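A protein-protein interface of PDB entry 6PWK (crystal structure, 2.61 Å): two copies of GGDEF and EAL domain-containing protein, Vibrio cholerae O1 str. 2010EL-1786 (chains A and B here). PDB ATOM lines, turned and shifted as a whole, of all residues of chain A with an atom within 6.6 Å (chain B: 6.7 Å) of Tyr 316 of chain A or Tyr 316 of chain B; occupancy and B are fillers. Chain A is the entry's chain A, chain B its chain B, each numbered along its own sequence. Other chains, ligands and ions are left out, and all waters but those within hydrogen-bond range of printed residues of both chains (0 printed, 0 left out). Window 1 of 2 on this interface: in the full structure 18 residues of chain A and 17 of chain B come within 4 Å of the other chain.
The guanidinium group (NH1) of Arg 285 of chain A lies within hydrogen-bond range of a ring nitrogen (ND1) of His 315 of chain B, at 3.3 Å.
OH of Tyr 316 of chain B lies close to OH of Tyr 316 of chain A (2.3 Å).
Pro 281 of chain A touches His 315 of chain B, and with the chains exchanged His 315 of chain A touches Pro 281 of chain B.
Pro 281 of chain A touches Tyr 316 of chain B, and with the chains exchanged Tyr 316 of chain A touches Pro 281 of chain B.
Arg 285 of chain A touches Ala 318 of chain B, and with the chains exchanged Ala 318 of chain A touches Arg 285 of chain B.
Tyr 316 of chain B touches its own counterpart, Tyr 316 of chain A.
Of chain B, only Pro 281 (3.5 Å) and Tyr 316 (2.3 Å) come within 4 Å of Tyr 316 of chain A.
Tyr 316 of chain B touches just these residues of chain A: Pro 281 (3.5 Å) and Tyr 316 (2.3 Å).
Printed residues of chain A within 4 Å of Leu 319 of chain B: Arg 285.
Of the printed residues of chain B, Ala 318 of chain A touches Arg 285 (3.4 Å).
Of the printed residues of chain B, His 315 of chain A touches Pro 281, Ser 282 and Arg 285.
Gln 280 of chain A touches none of the printed residues of chain B.
Phe 349 of chain B touches none of the printed residues of chain A.
The nearest residue of chain A that does not touch Tyr 316 of chain B is Ser 279 of chain A (4.4 Å).
Among the printed residues, no Asp or Glu carboxylate lies within 4 Å of a Lys or Arg side-chain nitrogen of the other chain.
CB of Pro 281 of chain A touches CB of His 315 of chain B, at 3.9 Å.
Ser 282 of chain A touches His 315 of chain B (CB to CD2, 3.4 Å).
Arg 285 of chain A touches Ala 318 of chain B (NE to CB, 3.5 Å).
CG of Arg 285 of chain A touches CD2 of Leu 319 of chain B, at 3.7 Å.
O of Pro 314 of chain A touches NH1 of Arg 285 of chain B, at 3.8 Å.
His 315 of chain A touches Pro 281 of chain B.
His 315 of chain A touches Ser 282 of chain B (ND1 to CB, 3.4 Å).
CG of Pro 281 of chain B touches CE2 of Tyr 316 of chain A, 3.5 Å away.
Leu 319 of chain A touches Pro 281 of chain B (CD1 to CB, 3.97 Å).
Leu 319 of chain A touches Arg 285 of chain B (CD2 to CG, 3.7 Å).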
ATOM      1  N   ILE A 278     -25.211  -3.960 -12.695  1.00  0.00           N
ATOM      2  CA  ILE A 278     -23.776  -4.072 -12.460  1.00  0.00           C
ATOM      3  C   ILE A 278     -23.409  -5.455 -11.929  1.00  0.00           C
ATOM      4  O   ILE A 278     -22.314  -5.964 -12.207  1.00  0.00           O
ATOM      5  CB  ILE A 278     -23.328  -2.936 -11.516  1.00  0.00           C
ATOM      6  CG1 ILE A 278     -23.046  -1.671 -12.330  1.00  0.00           C
ATOM      7  CG2 ILE A 278     -22.121  -3.336 -10.678  1.00  0.00           C
ATOM      8  CD1 ILE A 278     -22.816  -0.443 -11.492  1.00  0.00           C
ATOM      9  N   SER A 279     -24.311  -6.095 -11.188  1.00  0.00           N
ATOM     10  CA  SER A 279     -24.091  -7.454 -10.709  1.00  0.00           C
ATOM     11  C   SER A 279     -24.388  -8.512 -11.768  1.00  0.00           C
ATOM     12  O   SER A 279     -24.427  -9.703 -11.442  1.00  0.00           O
ATOM     13  CB  SER A 279     -24.934  -7.711  -9.457  1.00  0.00           C
ATOM     14  OG  SER A 279     -26.299  -7.410  -9.688  1.00  0.00           O
ATOM     15  N   GLN A 280     -24.599  -8.101 -13.022  1.00  0.00           N
ATOM     16  CA  GLN A 280     -24.824  -9.029 -14.119  1.00  0.00           C
ATOM     17  C   GLN A 280     -23.560  -9.109 -14.961  1.00  0.00           C
ATOM     18  O   GLN A 280     -23.236  -8.140 -15.665  1.00  0.00           O
ATOM     19  CB  GLN A 280     -26.008  -8.571 -14.973  1.00  0.00           C
ATOM     20  CG  GLN A 280     -27.010  -9.665 -15.313  1.00  0.00           C
ATOM     21  CD  GLN A 280     -27.796 -10.143 -14.106  1.00  0.00           C
ATOM     22  OE1 GLN A 280     -27.945  -9.422 -13.120  1.00  0.00           O
ATOM     23  NE2 GLN A 280     -28.303 -11.368 -14.179  1.00  0.00           N
ATOM     24  N   PRO A 281     -22.817 -10.217 -14.924  1.00  0.00           N
ATOM     25  CA  PRO A 281     -21.553 -10.272 -15.679  1.00  0.00           C
ATOM     26  C   PRO A 281     -21.728 -10.134 -17.182  1.00  0.00           C
ATOM     27  O   PRO A 281     -20.802  -9.670 -17.860  1.00  0.00           O
ATOM     28  CB  PRO A 281     -20.979 -11.644 -15.297  1.00  0.00           C
ATOM     29  CG  PRO A 281     -22.162 -12.443 -14.855  1.00  0.00           C
ATOM     30  CD  PRO A 281     -23.074 -11.462 -14.182  1.00  0.00           C
ATOM     31  N   SER A 282     -22.882 -10.525 -17.727  1.00  0.00           N
ATOM     32  CA  SER A 282     -23.140 -10.287 -19.144  1.00  0.00           C
ATOM     33  C   SER A 282     -23.199  -8.800 -19.455  1.00  0.00           C
ATOM     34  O   SER A 282     -22.777  -8.368 -20.534  1.00  0.00           O
ATOM     35  CB  SER A 282     -24.437 -10.974 -19.563  1.00  0.00           C
ATOM     36  OG  SER A 282     -25.510 -10.578 -18.730  1.00  0.00           O
ATOM     37  N   ILE A 284     -21.443  -6.549 -17.823  1.00  0.00           N
ATOM     38  CA  ILE A 284     -20.070  -6.057 -17.743  1.00  0.00           C
ATOM     39  C   ILE A 284     -19.318  -6.364 -19.032  1.00  0.00           C
ATOM     40  O   ILE A 284     -18.509  -5.555 -19.501  1.00  0.00           O
ATOM     41  CB  ILE A 284     -19.361  -6.648 -16.510  1.00  0.00           C
ATOM     42  CG1 ILE A 284     -20.157  -6.329 -15.242  1.00  0.00           C
ATOM     43  CG2 ILE A 284     -17.942  -6.106 -16.390  1.00  0.00           C
ATOM     44  CD1 ILE A 284     -19.486  -6.787 -13.964  1.00  0.00           C
ATOM     45  N   ARG A 285     -19.566  -7.536 -19.625  1.00  0.00           N
ATOM     46  CA  ARG A 285     -19.002  -7.823 -20.941  1.00  0.00           C
ATOM     47  C   ARG A 285     -19.619  -6.933 -22.008  1.00  0.00           C
ATOM     48  O   ARG A 285     -18.922  -6.467 -22.917  1.00  0.00           O
ATOM     49  CB  ARG A 285     -19.218  -9.293 -21.304  1.00  0.00           C
ATOM     50  CG  ARG A 285     -18.369 -10.283 -20.536  1.00  0.00           C
ATOM     51  CD  ARG A 285     -18.598 -11.685 -21.076  1.00  0.00           C
ATOM     52  NE  ARG A 285     -18.097 -11.836 -22.441  1.00  0.00           N
ATOM     53  CZ  ARG A 285     -18.449 -12.819 -23.264  1.00  0.00           C
ATOM     54  NH1 ARG A 285     -19.317 -13.740 -22.867  1.00  0.00           N
ATOM     55  NH2 ARG A 285     -17.941 -12.878 -24.487  1.00  0.00           N
ATOM     56  N   GLU A 313     -21.641  -4.215  -3.438  1.00  0.00           N
ATOM     57  CA  GLU A 313     -21.097  -5.039  -4.518  1.00  0.00           C
ATOM     58  C   GLU A 313     -19.801  -4.426  -5.039  1.00  0.00           C
ATOM     59  O   GLU A 313     -19.714  -4.025  -6.203  1.00  0.00           O
ATOM     60  CB  GLU A 313     -22.117  -5.190  -5.647  1.00  0.00           C
ATOM     61  CG  GLU A 313     -23.464  -5.755  -5.217  1.00  0.00           C
ATOM     62  CD  GLU A 313     -23.397  -7.229  -4.861  1.00  0.00           C
ATOM     63  OE1 GLU A 313     -22.368  -7.871  -5.159  1.00  0.00           O
ATOM     64  OE2 GLU A 313     -24.377  -7.746  -4.284  1.00  0.00           O
ATOM     65  N   PRO A 314     -18.763  -4.343  -4.199  1.00  0.00           N
ATOM     66  CA  PRO A 314     -17.533  -3.667  -4.640  1.00  0.00           C
ATOM     67  C   PRO A 314     -16.828  -4.387  -5.773  1.00  0.00           C
ATOM     68  O   PRO A 314     -16.187  -3.733  -6.606  1.00  0.00           O
ATOM     69  CB  PRO A 314     -16.662  -3.640  -3.373  1.00  0.00           C
ATOM     70  CG  PRO A 314     -17.567  -4.045  -2.245  1.00  0.00           C
ATOM     71  CD  PRO A 314     -18.613  -4.919  -2.853  1.00  0.00           C
ATOM     72  N   HIS A 315     -16.932  -5.716  -5.834  1.00  0.00           N
ATOM     73  CA  HIS A 315     -16.184  -6.472  -6.830  1.00  0.00           C
ATOM     74  C   HIS A 315     -16.869  -6.445  -8.190  1.00  0.00           C
ATOM     75  O   HIS A 315     -16.198  -6.284  -9.215  1.00  0.00           O
ATOM     76  CB  HIS A 315     -15.980  -7.902  -6.337  1.00  0.00           C
ATOM     77  CG  HIS A 315     -15.340  -7.977  -4.986  1.00  0.00           C
ATOM     78  ND1 HIS A 315     -16.013  -8.411  -3.864  1.00  0.00           N
ATOM     79  CD2 HIS A 315     -14.094  -7.644  -4.572  1.00  0.00           C
ATOM     80  CE1 HIS A 315     -15.205  -8.357  -2.820  1.00  0.00           C
ATOM     81  NE2 HIS A 315     -14.036  -7.895  -3.223  1.00  0.00           N
ATOM     82  N   TYR A 316     -18.195  -6.602  -8.224  1.00  0.00           N
ATOM     83  CA  TYR A 316     -18.927  -6.348  -9.461  1.00  0.00           C
ATOM     84  C   TYR A 316     -18.701  -4.921  -9.941  1.00  0.00           C
ATOM     85  O   TYR A 316     -18.498  -4.682 -11.137  1.00  0.00           O
ATOM     86  CB  TYR A 316     -20.423  -6.597  -9.262  1.00  0.00           C
ATOM     87  CG  TYR A 316     -20.846  -8.047  -9.254  1.00  0.00           C
ATOM     88  CD1 TYR A 316     -20.778  -8.819 -10.408  1.00  0.00           C
ATOM     89  CD2 TYR A 316     -21.352  -8.634  -8.102  1.00  0.00           C
ATOM     90  CE1 TYR A 316     -21.181 -10.143 -10.405  1.00  0.00           C
ATOM     91  CE2 TYR A 316     -21.757  -9.952  -8.091  1.00  0.00           C
ATOM     92  CZ  TYR A 316     -21.670 -10.702  -9.243  1.00  0.00           C
ATOM     93  OH  TYR A 316     -22.074 -12.017  -9.227  1.00  0.00           O
ATOM     94  N   THR A 317     -18.731  -3.959  -9.016  1.00  0.00           N
ATOM     95  CA  THR A 317     -18.579  -2.557  -9.389  1.00  0.00           C
ATOM     96  C   THR A 317     -17.186  -2.280  -9.941  1.00  0.00           C
ATOM     97  O   THR A 317     -17.038  -1.556 -10.934  1.00  0.00           O
ATOM     98  CB  THR A 317     -18.868  -1.662  -8.184  1.00  0.00           C
ATOM     99  OG1 THR A 317     -20.095  -2.072  -7.567  1.00  0.00           O
ATOM    100  CG2 THR A 317     -18.988  -0.210  -8.613  1.00  0.00           C
ATOM    101  N   ALA A 318     -16.151  -2.846  -9.315  1.00  0.00           N
ATOM    102  CA  ALA A 318     -14.793  -2.632  -9.802  1.00  0.00           C
ATOM    103  C   ALA A 318     -14.593  -3.251 -11.178  1.00  0.00           C
ATOM    104  O   ALA A 318     -13.869  -2.697 -12.013  1.00  0.00           O
ATOM    105  CB  ALA A 318     -13.779  -3.194  -8.805  1.00  0.00           C
ATOM    106  N   LEU A 319     -15.223  -4.399 -11.436  1.00  0.00           N
ATOM    107  CA  LEU A 319     -15.160  -4.981 -12.772  1.00  0.00           C
ATOM    108  C   LEU A 319     -15.853  -4.083 -13.788  1.00  0.00           C
ATOM    109  O   LEU A 319     -15.373  -3.923 -14.917  1.00  0.00           O
ATOM    110  CB  LEU A 319     -15.783  -6.377 -12.775  1.00  0.00           C
ATOM    111  CG  LEU A 319     -15.075  -7.442 -11.936  1.00  0.00           C
ATOM    112  CD1 LEU A 319     -15.770  -8.788 -12.080  1.00  0.00           C
ATOM    113  CD2 LEU A 319     -13.606  -7.544 -12.313  1.00  0.00           C
ATOM    114  N   PHE A 320     -16.982  -3.485 -13.404  1.00  0.00           N
ATOM    115  CA  PHE A 320     -17.666  -2.557 -14.298  1.00  0.00           C
ATOM    116  C   PHE A 320     -16.855  -1.282 -14.493  1.00  0.00           C
ATOM    117  O   PHE A 320     -16.733  -0.783 -15.617  1.00  0.00           O
ATOM    118  CB  PHE A 320     -19.057  -2.235 -13.752  1.00  0.00           C
ATOM    119  CG  PHE A 320     -19.816  -1.236 -14.576  1.00  0.00           C
ATOM    120  CD1 PHE A 320     -20.482  -1.629 -15.724  1.00  0.00           C
ATOM    121  CD2 PHE A 320     -19.866   0.098 -14.202  1.00  0.00           C
ATOM    122  CE1 PHE A 320     -21.180  -0.712 -16.486  1.00  0.00           C
ATOM    123  CE2 PHE A 320     -20.563   1.019 -14.959  1.00  0.00           C
ATOM    124  CZ  PHE A 320     -21.221   0.614 -16.103  1.00  0.00           C
ATOM    125  N   CYS A 321     -16.288  -0.747 -13.408  1.00  0.00           N
ATOM    126  CA  CYS A 321     -15.513   0.486 -13.508  1.00  0.00           C
ATOM    127  C   CYS A 321     -14.268   0.295 -14.363  1.00  0.00           C
ATOM    128  O   CYS A 321     -13.885   1.194 -15.121  1.00  0.00           O
ATOM    129  CB  CYS A 321     -15.137   0.983 -12.112  1.00  0.00           C
ATOM    130  SG  CYS A 321     -16.525   1.631 -11.152  1.00  0.00           S
ATOM    131  N   ILE B 278     -14.927 -19.259 -10.067  1.00  0.00           N
ATOM    132  CA  ILE B 278     -14.935 -18.354 -11.208  1.00  0.00           C
ATOM    133  C   ILE B 278     -16.183 -17.479 -11.206  1.00  0.00           C
ATOM    134  O   ILE B 278     -16.161 -16.347 -11.712  1.00  0.00           O
ATOM    135  CB  ILE B 278     -14.789 -19.177 -12.508  1.00  0.00           C
ATOM    136  CG1 ILE B 278     -13.297 -19.392 -12.812  1.00  0.00           C
ATOM    137  CG2 ILE B 278     -15.508 -18.529 -13.686  1.00  0.00           C
ATOM    138  CD1 ILE B 278     -13.034 -20.376 -13.931  1.00  0.00           C
ATOM    139  N   SER B 279     -17.273 -17.955 -10.609  1.00  0.00           N
ATOM    140  CA  SER B 279     -18.486 -17.157 -10.485  1.00  0.00           C
ATOM    141  C   SER B 279     -18.454 -16.214  -9.284  1.00  0.00           C
ATOM    142  O   SER B 279     -19.488 -15.635  -8.940  1.00  0.00           O
ATOM    143  CB  SER B 279     -19.710 -18.072 -10.401  1.00  0.00           C
ATOM    144  OG  SER B 279     -19.593 -18.990  -9.332  1.00  0.00           O
ATOM    145  N   GLN B 280     -17.295 -16.050  -8.640  1.00  0.00           N
ATOM    146  CA  GLN B 280     -17.145 -15.096  -7.551  1.00  0.00           C
ATOM    147  C   GLN B 280     -16.371 -13.893  -8.065  1.00  0.00           C
ATOM    148  O   GLN B 280     -15.173 -14.024  -8.362  1.00  0.00           O
ATOM    149  CB  GLN B 280     -16.421 -15.734  -6.366  1.00  0.00           C
ATOM    150  CG  GLN B 280     -17.029 -15.407  -5.010  1.00  0.00           C
ATOM    151  CD  GLN B 280     -18.364 -16.092  -4.790  1.00  0.00           C
ATOM    152  OE1 GLN B 280     -18.660 -17.115  -5.409  1.00  0.00           O
ATOM    153  NE2 GLN B 280     -19.180 -15.528  -3.908  1.00  0.00           N
ATOM    154  N   PRO B 281     -16.992 -12.717  -8.196  1.00  0.00           N
ATOM    155  CA  PRO B 281     -16.276 -11.575  -8.793  1.00  0.00           C
ATOM    156  C   PRO B 281     -15.068 -11.121  -7.991  1.00  0.00           C
ATOM    157  O   PRO B 281     -14.126 -10.569  -8.574  1.00  0.00           O
ATOM    158  CB  PRO B 281     -17.354 -10.481  -8.863  1.00  0.00           C
ATOM    159  CG  PRO B 281     -18.386 -10.888  -7.863  1.00  0.00           C
ATOM    160  CD  PRO B 281     -18.389 -12.388  -7.869  1.00  0.00           C
ATOM    161  N   SER B 282     -15.064 -11.331  -6.672  1.00  0.00           N
ATOM    162  CA  SER B 282     -13.875 -11.022  -5.886  1.00  0.00           C
ATOM    163  C   SER B 282     -12.687 -11.871  -6.322  1.00  0.00           C
ATOM    164  O   SER B 282     -11.541 -11.408  -6.279  1.00  0.00           O
ATOM    165  CB  SER B 282     -14.162 -11.223  -4.397  1.00  0.00           C
ATOM    166  OG  SER B 282     -14.576 -12.553  -4.134  1.00  0.00           O
ATOM    167  N   ILE B 284     -12.253 -12.935  -9.449  1.00  0.00           N
ATOM    168  CA  ILE B 284     -11.830 -12.429 -10.753  1.00  0.00           C
ATOM    169  C   ILE B 284     -10.972 -11.179 -10.589  1.00  0.00           C
ATOM    170  O   ILE B 284     -10.022 -10.959 -11.349  1.00  0.00           O
ATOM    171  CB  ILE B 284     -13.053 -12.169 -11.653  1.00  0.00           C
ATOM    172  CG1 ILE B 284     -13.918 -13.428 -11.751  1.00  0.00           C
ATOM    173  CG2 ILE B 284     -12.617 -11.724 -13.043  1.00  0.00           C
ATOM    174  CD1 ILE B 284     -15.108 -13.278 -12.677  1.00  0.00           C
ATOM    175  N   ARG B 285     -11.294 -10.337  -9.604  1.00  0.00           N
ATOM    176  CA  ARG B 285     -10.423  -9.208  -9.291  1.00  0.00           C
ATOM    177  C   ARG B 285      -9.101  -9.681  -8.706  1.00  0.00           C
ATOM    178  O   ARG B 285      -8.037  -9.150  -9.046  1.00  0.00           O
ATOM    179  CB  ARG B 285     -11.108  -8.263  -8.307  1.00  0.00           C
ATOM    180  CG  ARG B 285     -12.228  -7.431  -8.878  1.00  0.00           C
ATOM    181  CD  ARG B 285     -12.711  -6.451  -7.826  1.00  0.00           C
ATOM    182  NE  ARG B 285     -11.664  -5.508  -7.441  1.00  0.00           N
ATOM    183  CZ  ARG B 285     -11.707  -4.748  -6.351  1.00  0.00           C
ATOM    184  NH1 ARG B 285     -12.743  -4.826  -5.527  1.00  0.00           N
ATOM    185  NH2 ARG B 285     -10.711  -3.914  -6.080  1.00  0.00           N
ATOM    186  N   CYS B 309     -18.051 -24.703 -16.657  1.00  0.00           N
ATOM    187  CA  CYS B 309     -17.964 -23.249 -16.562  1.00  0.00           C
ATOM    188  C   CYS B 309     -18.313 -22.590 -17.887  1.00  0.00           C
ATOM    189  O   CYS B 309     -19.101 -21.640 -17.935  1.00  0.00           O
ATOM    190  CB  CYS B 309     -16.563 -22.829 -16.122  1.00  0.00           C
ATOM    191  SG  CYS B 309     -16.265 -22.884 -14.355  1.00  0.00           S
ATOM    192  N   GLU B 313     -21.677 -21.005 -17.140  1.00  0.00           N
ATOM    193  CA  GLU B 313     -21.301 -19.691 -16.619  1.00  0.00           C
ATOM    194  C   GLU B 313     -20.373 -18.989 -17.606  1.00  0.00           C
ATOM    195  O   GLU B 313     -19.233 -18.650 -17.274  1.00  0.00           O
ATOM    196  CB  GLU B 313     -20.635 -19.840 -15.252  1.00  0.00           C
ATOM    197  CG  GLU B 313     -21.222 -18.975 -14.154  1.00  0.00           C
ATOM    198  CD  GLU B 313     -22.676 -19.286 -13.868  1.00  0.00           C
ATOM    199  OE1 GLU B 313     -23.498 -18.346 -13.879  1.00  0.00           O
ATOM    200  OE2 GLU B 313     -22.996 -20.470 -13.637  1.00  0.00           O
ATOM    201  N   PRO B 314     -20.835 -18.747 -18.839  1.00  0.00           N
ATOM    202  CA  PRO B 314     -19.911 -18.237 -19.865  1.00  0.00           C
ATOM    203  C   PRO B 314     -19.451 -16.810 -19.621  1.00  0.00           C
ATOM    204  O   PRO B 314     -18.318 -16.471 -19.984  1.00  0.00           O
ATOM    205  CB  PRO B 314     -20.730 -18.352 -21.157  1.00  0.00           C
ATOM    206  CG  PRO B 314     -22.138 -18.212 -20.707  1.00  0.00           C
ATOM    207  CD  PRO B 314     -22.211 -18.871 -19.354  1.00  0.00           C
ATOM    208  N   HIS B 315     -20.290 -15.963 -19.017  1.00  0.00           N
ATOM    209  CA  HIS B 315     -19.915 -14.566 -18.828  1.00  0.00           C
ATOM    210  C   HIS B 315     -18.890 -14.400 -17.713  1.00  0.00           C
ATOM    211  O   HIS B 315     -17.932 -13.634 -17.863  1.00  0.00           O
ATOM    212  CB  HIS B 315     -21.162 -13.724 -18.558  1.00  0.00           C
ATOM    213  CG  HIS B 315     -22.210 -13.847 -19.619  1.00  0.00           C
ATOM    214  ND1 HIS B 315     -21.974 -13.518 -20.936  1.00  0.00           N
ATOM    215  CD2 HIS B 315     -23.493 -14.273 -19.561  1.00  0.00           C
ATOM    216  CE1 HIS B 315     -23.068 -13.732 -21.643  1.00  0.00           C
ATOM    217  NE2 HIS B 315     -24.005 -14.189 -20.832  1.00  0.00           N
ATOM    218  N   TYR B 316     -19.074 -15.096 -16.589  1.00  0.00           N
ATOM    219  CA  TYR B 316     -18.036 -15.115 -15.561  1.00  0.00           C
ATOM    220  C   TYR B 316     -16.739 -15.692 -16.113  1.00  0.00           C
ATOM    221  O   TYR B 316     -15.651 -15.159 -15.861  1.00  0.00           O
ATOM    222  CB  TYR B 316     -18.489 -15.930 -14.349  1.00  0.00           C
ATOM    223  CG  TYR B 316     -19.515 -15.267 -13.453  1.00  0.00           C
ATOM    224  CD1 TYR B 316     -19.165 -14.213 -12.619  1.00  0.00           C
ATOM    225  CD2 TYR B 316     -20.824 -15.725 -13.413  1.00  0.00           C
ATOM    226  CE1 TYR B 316     -20.101 -13.618 -11.788  1.00  0.00           C
ATOM    227  CE2 TYR B 316     -21.763 -15.142 -12.586  1.00  0.00           C
ATOM    228  CZ  TYR B 316     -21.397 -14.089 -11.777  1.00  0.00           C
ATOM    229  OH  TYR B 316     -22.331 -13.506 -10.954  1.00  0.00           O
ATOM    230  N   THR B 317     -16.840 -16.784 -16.874  1.00  0.00           N
ATOM    231  CA  THR B 317     -15.650 -17.439 -17.405  1.00  0.00           C
ATOM    232  C   THR B 317     -14.916 -16.541 -18.391  1.00  0.00           C
ATOM    233  O   THR B 317     -13.680 -16.519 -18.418  1.00  0.00           O
ATOM    234  CB  THR B 317     -16.035 -18.763 -18.068  1.00  0.00           C
ATOM    235  OG1 THR B 317     -16.865 -19.519 -17.179  1.00  0.00           O
ATOM    236  CG2 THR B 317     -14.794 -19.574 -18.404  1.00  0.00           C
ATOM    237  N   ALA B 318     -15.659 -15.792 -19.209  1.00  0.00           N
ATOM    238  CA  ALA B 318     -15.021 -14.877 -20.150  1.00  0.00           C
ATOM    239  C   ALA B 318     -14.282 -13.763 -19.419  1.00  0.00           C
ATOM    240  O   ALA B 318     -13.202 -13.339 -19.847  1.00  0.00           O
ATOM    241  CB  ALA B 318     -16.062 -14.296 -21.106  1.00  0.00           C
ATOM    242  N   LEU B 319     -14.850 -13.272 -18.315  1.00  0.00           N
ATOM    243  CA  LEU B 319     -14.150 -12.272 -17.515  1.00  0.00           C
ATOM    244  C   LEU B 319     -12.899 -12.859 -16.876  1.00  0.00           C
ATOM    245  O   LEU B 319     -11.857 -12.196 -16.810  1.00  0.00           O
ATOM    246  CB  LEU B 319     -15.084 -11.705 -16.445  1.00  0.00           C
ATOM    247  CG  LEU B 319     -16.308 -10.929 -16.933  1.00  0.00           C
ATOM    248  CD1 LEU B 319     -17.127 -10.440 -15.749  1.00  0.00           C
ATOM    249  CD2 LEU B 319     -15.891  -9.767 -17.819  1.00  0.00           C
ATOM    250  N   PHE B 320     -12.981 -14.103 -16.404  1.00  0.00           N
ATOM    251  CA  PHE B 320     -11.807 -14.754 -15.833  1.00  0.00           C
ATOM    252  C   PHE B 320     -10.763 -15.045 -16.904  1.00  0.00           C
ATOM    253  O   PHE B 320      -9.566 -14.821 -16.689  1.00  0.00           O
ATOM    254  CB  PHE B 320     -12.219 -16.040 -15.118  1.00  0.00           C
ATOM    255  CG  PHE B 320     -11.066 -16.813 -14.551  1.00  0.00           C
ATOM    256  CD1 PHE B 320     -10.522 -16.468 -13.324  1.00  0.00           C
ATOM    257  CD2 PHE B 320     -10.526 -17.886 -15.241  1.00  0.00           C
ATOM    258  CE1 PHE B 320      -9.459 -17.177 -12.800  1.00  0.00           C
ATOM    259  CE2 PHE B 320      -9.464 -18.598 -14.723  1.00  0.00           C
ATOM    260  CZ  PHE B 320      -8.929 -18.243 -13.501  1.00  0.00           C
ATOM    261  N   CYS B 321     -11.197 -15.544 -18.064  1.00  0.00           N
ATOM    262  CA  CYS B 321     -10.257 -15.877 -19.131  1.00  0.00           C
ATOM    263  C   CYS B 321      -9.549 -14.635 -19.657  1.00  0.00           C
ATOM    264  O   CYS B 321      -8.351 -14.675 -19.958  1.00  0.00           O
ATOM    265  CB  CYS B 321     -10.979 -16.596 -20.269  1.00  0.00           C
ATOM    266  SG  CYS B 321     -11.461 -18.292 -19.897  1.00  0.00           S
ATOM    267  N   PHE B 349     -13.964 -19.054 -27.158  1.00  0.00           N
ATOM    268  CA  PHE B 349     -12.930 -18.885 -26.144  1.00  0.00           C
ATOM    269  C   PHE B 349     -11.528 -19.194 -26.650  1.00  0.00           C
ATOM    270  O   PHE B 349     -10.566 -18.574 -26.181  1.00  0.00           O
ATOM    271  CB  PHE B 349     -13.241 -19.761 -24.928  1.00  0.00           C
ATOM    272  CG  PHE B 349     -14.346 -19.224 -24.065  1.00  0.00           C
ATOM    273  CD1 PHE B 349     -15.673 -19.454 -24.388  1.00  0.00           C
ATOM    274  CD2 PHE B 349     -14.056 -18.487 -22.929  1.00  0.00           C
ATOM    275  CE1 PHE B 349     -16.690 -18.959 -23.596  1.00  0.00           C
ATOM    276  CE2 PHE B 349     -15.069 -17.990 -22.131  1.00  0.00           C
ATOM    277  CZ  PHE B 349     -16.387 -18.226 -22.465  1.00  0.00           C
